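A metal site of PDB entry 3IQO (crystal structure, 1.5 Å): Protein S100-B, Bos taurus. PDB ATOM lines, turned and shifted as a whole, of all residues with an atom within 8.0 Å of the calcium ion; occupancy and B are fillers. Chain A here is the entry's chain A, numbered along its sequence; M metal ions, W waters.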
ATOM      1  N   LYS A  27       7.717 -20.234   9.003  1.00  0.00           N
ATOM      2  CA  LYS A  27       6.691 -20.966   9.735  1.00  0.00           C
ATOM      3  C   LYS A  27       6.108 -22.033   8.845  1.00  0.00           C
ATOM      4  O   LYS A  27       6.101 -21.884   7.608  1.00  0.00           O
ATOM      5  CB  LYS A  27       5.578 -20.046  10.226  1.00  0.00           C
ATOM      6  CG  LYS A  27       6.077 -18.903  11.106  1.00  0.00           C
ATOM      7  CD  LYS A  27       4.970 -18.223  11.864  1.00  0.00           C
ATOM      8  CE  LYS A  27       5.521 -17.084  12.701  1.00  0.00           C
ATOM      9  NZ  LYS A  27       6.013 -15.961  11.836  1.00  0.00           N
ATOM     10  N   LEU A  28       5.602 -23.094   9.478  1.00  0.00           N
ATOM     11  CA  LEU A  28       4.890 -24.185   8.800  1.00  0.00           C
ATOM     12  C   LEU A  28       3.380 -23.929   8.819  1.00  0.00           C
ATOM     13  O   LEU A  28       2.750 -23.858   9.883  1.00  0.00           O
ATOM     14  CB  LEU A  28       5.151 -25.534   9.480  1.00  0.00           C
ATOM     15  CG  LEU A  28       6.597 -26.028   9.523  1.00  0.00           C
ATOM     16  CD1 LEU A  28       6.719 -27.122  10.610  1.00  0.00           C
ATOM     17  CD2 LEU A  28       7.090 -26.587   8.195  1.00  0.00           C
ATOM     18  N   MET A  58      -2.263 -29.377  14.067  1.00  0.00           N
ATOM     19  CA  MET A  58      -1.885 -27.940  14.100  1.00  0.00           C
ATOM     20  C   MET A  58      -2.399 -27.265  15.351  1.00  0.00           C
ATOM     21  O   MET A  58      -1.672 -26.524  16.001  1.00  0.00           O
ATOM     22  CB  MET A  58      -2.359 -27.176  12.868  1.00  0.00           C
ATOM     23  CG  MET A  58      -1.924 -25.687  12.914  1.00  0.00           C
ATOM     24  SD  MET A  58      -0.100 -25.472  12.836  1.00  0.00           S
ATOM     25  CE  MET A  58       0.152 -25.650  11.073  1.00  0.00           C
ATOM     26  N   LEU A  61      -0.072 -28.166  18.258  1.00  0.00           N
ATOM     27  CA  LEU A  61       1.272 -27.585  18.208  1.00  0.00           C
ATOM     28  C   LEU A  61       1.293 -26.067  18.260  1.00  0.00           C
ATOM     29  O   LEU A  61       2.265 -25.491  18.715  1.00  0.00           O
ATOM     30  CB  LEU A  61       2.002 -28.057  16.935  1.00  0.00           C
ATOM     31  CG  LEU A  61       2.091 -29.577  16.706  1.00  0.00           C
ATOM     32  CD1 LEU A  61       2.959 -29.888  15.511  1.00  0.00           C
ATOM     33  CD2 LEU A  61       2.609 -30.365  17.948  1.00  0.00           C
ATOM     34  N   ASP A  62       0.231 -25.415  17.792  1.00  0.00           N
ATOM     35  CA  ASP A  62       0.182 -23.968  17.711  1.00  0.00           C
ATOM     36  C   ASP A  62      -0.125 -23.301  19.062  1.00  0.00           C
ATOM     37  O   ASP A  62      -1.257 -22.839  19.312  1.00  0.00           O
ATOM     38  CB  ASP A  62      -0.852 -23.539  16.662  1.00  0.00           C
ATOM     39  CG  ASP A  62      -0.867 -22.057  16.414  1.00  0.00           C
ATOM     40  OD1 ASP A  62       0.181 -21.379  16.627  1.00  0.00           O
ATOM     41  OD2 ASP A  62      -1.923 -21.586  15.934  1.00  0.00           O
ATOM     42  N   SER A  63       0.921 -23.190  19.894  1.00  0.00           N
ATOM     43  CA  SER A  63       0.765 -22.585  21.213  1.00  0.00           C
ATOM     44  C   SER A  63       0.383 -21.115  21.169  1.00  0.00           C
ATOM     45  O   SER A  63      -0.376 -20.648  22.032  1.00  0.00           O
ATOM     46  CB  SER A  63       2.038 -22.750  22.042  1.00  0.00           C
ATOM     47  OG  SER A  63       2.281 -24.113  22.298  1.00  0.00           O
ATOM     48  N   ASP A  64       0.910 -20.355  20.211  1.00  0.00           N
ATOM     49  CA  ASP A  64       0.654 -18.892  20.163  1.00  0.00           C
ATOM     50  C   ASP A  64      -0.564 -18.470  19.341  1.00  0.00           C
ATOM     51  O   ASP A  64      -0.831 -17.278  19.180  1.00  0.00           O
ATOM     52  CB  ASP A  64       1.914 -18.083  19.770  1.00  0.00           C
ATOM     53  CG  ASP A  64       2.415 -18.377  18.338  1.00  0.00           C
ATOM     54  OD1 ASP A  64       1.660 -18.911  17.489  1.00  0.00           O
ATOM     55  OD2 ASP A  64       3.599 -18.045  18.056  1.00  0.00           O
ATOM     56  N   GLY A  65      -1.281 -19.451  18.791  1.00  0.00           N
ATOM     57  CA  GLY A  65      -2.556 -19.224  18.114  1.00  0.00           C
ATOM     58  C   GLY A  65      -2.627 -18.506  16.770  1.00  0.00           C
ATOM     59  O   GLY A  65      -3.728 -18.166  16.319  1.00  0.00           O
ATOM     60  N   ASP A  66      -1.499 -18.306  16.103  1.00  0.00           N
ATOM     61  CA  ASP A  66      -1.501 -17.681  14.770  1.00  0.00           C
ATOM     62  C   ASP A  66      -1.822 -18.643  13.602  1.00  0.00           C
ATOM     63  O   ASP A  66      -1.811 -18.247  12.425  1.00  0.00           O
ATOM     64  CB  ASP A  66      -0.178 -16.934  14.513  1.00  0.00           C
ATOM     65  CG  ASP A  66       1.014 -17.857  14.406  1.00  0.00           C
ATOM     66  OD1 ASP A  66       0.852 -19.100  14.529  1.00  0.00           O
ATOM     67  OD2 ASP A  66       2.140 -17.359  14.192  1.00  0.00           O
ATOM     68  N   GLY A  67      -2.120 -19.892  13.916  1.00  0.00           N
ATOM     69  CA  GLY A  67      -2.492 -20.875  12.905  1.00  0.00           C
ATOM     70  C   GLY A  67      -1.332 -21.534  12.164  1.00  0.00           C
ATOM     71  O   GLY A  67      -1.556 -22.273  11.192  1.00  0.00           O
ATOM     72  N   GLU A  68      -0.099 -21.263  12.608  1.00  0.00           N
ATOM     73  CA  GLU A  68       1.092 -21.796  11.954  1.00  0.00           C
ATOM     74  C   GLU A  68       2.049 -22.307  13.010  1.00  0.00           C
ATOM     75  O   GLU A  68       1.915 -21.966  14.180  1.00  0.00           O
ATOM     76  CB  GLU A  68       1.801 -20.738  11.088  1.00  0.00           C
ATOM     77  CG  GLU A  68       0.931 -20.226   9.923  1.00  0.00           C
ATOM     78  CD  GLU A  68       1.745 -19.818   8.719  1.00  0.00           C
ATOM     79  OE1 GLU A  68       2.864 -20.350   8.511  1.00  0.00           O
ATOM     80  OE2 GLU A  68       1.250 -18.979   7.939  1.00  0.00           O
ATOM     81  N   CYS A  69       2.992 -23.149  12.601  1.00  0.00           N
ATOM     82  CA  CYS A  69       3.950 -23.725  13.522  1.00  0.00           C
ATOM     83  C   CYS A  69       5.311 -23.033  13.310  1.00  0.00           C
ATOM     84  O   CYS A  69       5.938 -23.172  12.247  1.00  0.00           O
ATOM     85  CB  CYS A  69       4.043 -25.254  13.302  1.00  0.00           C
ATOM     86  SG  CYS A  69       5.175 -26.089  14.440  1.00  0.00           S
ATOM     87  N   ASP A  70       5.740 -22.256  14.298  1.00  0.00           N
ATOM     88  CA  ASP A  70       7.054 -21.599  14.179  1.00  0.00           C
ATOM     89  C   ASP A  70       8.157 -22.511  14.698  1.00  0.00           C
ATOM     90  O   ASP A  70       7.905 -23.676  15.097  1.00  0.00           O
ATOM     91  CB  ASP A  70       7.075 -20.196  14.831  1.00  0.00           C
ATOM     92  CG  ASP A  70       6.915 -20.230  16.356  1.00  0.00           C
ATOM     93  OD1 ASP A  70       7.147 -21.265  17.017  1.00  0.00           O
ATOM     94  OD2 ASP A  70       6.574 -19.178  16.917  1.00  0.00           O
ATOM     95  N   PHE A  71       9.399 -22.014  14.682  1.00  0.00           N
ATOM     96  CA  PHE A  71      10.481 -22.893  15.063  1.00  0.00           C
ATOM     97  C   PHE A  71      10.392 -23.395  16.499  1.00  0.00           C
ATOM     98  O   PHE A  71      10.653 -24.575  16.770  1.00  0.00           O
ATOM     99  CB  PHE A  71      11.850 -22.284  14.767  1.00  0.00           C
ATOM    100  CG  PHE A  71      12.969 -23.300  14.898  1.00  0.00           C
ATOM    101  CD1 PHE A  71      13.059 -24.358  13.990  1.00  0.00           C
ATOM    102  CD2 PHE A  71      13.863 -23.252  15.966  1.00  0.00           C
ATOM    103  CE1 PHE A  71      14.055 -25.319  14.108  1.00  0.00           C
ATOM    104  CE2 PHE A  71      14.857 -24.200  16.087  1.00  0.00           C
ATOM    105  CZ  PHE A  71      14.946 -25.239  15.164  1.00  0.00           C
ATOM    106  N   GLU A  73       7.707 -23.828  18.292  1.00  0.00           N
ATOM    107  CA  GLU A  73       6.601 -24.792  18.369  1.00  0.00           C
ATOM    108  C   GLU A  73       7.032 -26.123  17.746  1.00  0.00           C
ATOM    109  O   GLU A  73       6.641 -27.189  18.224  1.00  0.00           O
ATOM    110  CB  GLU A  73       5.349 -24.212  17.676  1.00  0.00           C
ATOM    111  CG  GLU A  73       4.720 -23.103  18.491  1.00  0.00           C
ATOM    112  CD  GLU A  73       3.754 -22.227  17.705  1.00  0.00           C
ATOM    113  OE1 GLU A  73       3.825 -22.208  16.452  1.00  0.00           O
ATOM    114  OE2 GLU A  73       2.931 -21.530  18.334  1.00  0.00           O
ATOM    115  N   PHE A  74       7.821 -26.060  16.691  1.00  0.00           N
ATOM    116  CA  PHE A  74       8.359 -27.254  16.060  1.00  0.00           C
ATOM    117  C   PHE A  74       9.277 -28.006  17.048  1.00  0.00           C
ATOM    118  O   PHE A  74       9.218 -29.241  17.149  1.00  0.00           O
ATOM    119  CB  PHE A  74       9.112 -26.911  14.773  1.00  0.00           C
ATOM    120  CG  PHE A  74       9.796 -28.081  14.148  1.00  0.00           C
ATOM    121  CD1 PHE A  74       9.031 -29.093  13.531  1.00  0.00           C
ATOM    122  CD2 PHE A  74      11.193 -28.179  14.123  1.00  0.00           C
ATOM    123  CE1 PHE A  74       9.671 -30.179  12.925  1.00  0.00           C
ATOM    124  CE2 PHE A  74      11.830 -29.275  13.522  1.00  0.00           C
ATOM    125  CZ  PHE A  74      11.064 -30.268  12.921  1.00  0.00           C
HETATM  126 CA    CA M   1       2.191 -20.569  16.013  1.00  0.00          CA
HETATM  127  O   HOH W   1       3.909 -19.022  15.221  1.00  0.00           O
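Within 4 Å of the calcium ion: Asp 62, Asp 64, Asp 66, Glu 68 and Glu 73.
The calcium ion is bound by the side-chain carboxylate (OD1) of Asp 62 (2.3 Å), the side-chain carboxylate (OD1) of Asp 64 (2.3 Å), the backbone carbonyl oxygen (O) of Glu 68 (2.3 Å), the side-chain carboxylate (OE1) of Glu 73 (2.4 Å), water W1 (2.4 Å), the side-chain carboxylate (OD1) of Asp 66 (2.5 Å) and the side-chain carboxylate (OE2) of Glu 73 (2.6 Å).
The side-chain carboxylate of Asp 62 lies close to the backbone NH of Gly 65.
OD2 of Asp 62 lies within hydrogen-bond range of N of Gly 67, at 2.6 Å.
The backbone NH of Glu 73 is in hydrogen-bond range of the side-chain carboxylate of Asp 70 (2.9 Å).
The side-chain carboxylate (OE2) of Glu 73 sits close to the backbone NH (N) of Ser 63, 3.0 Å away.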
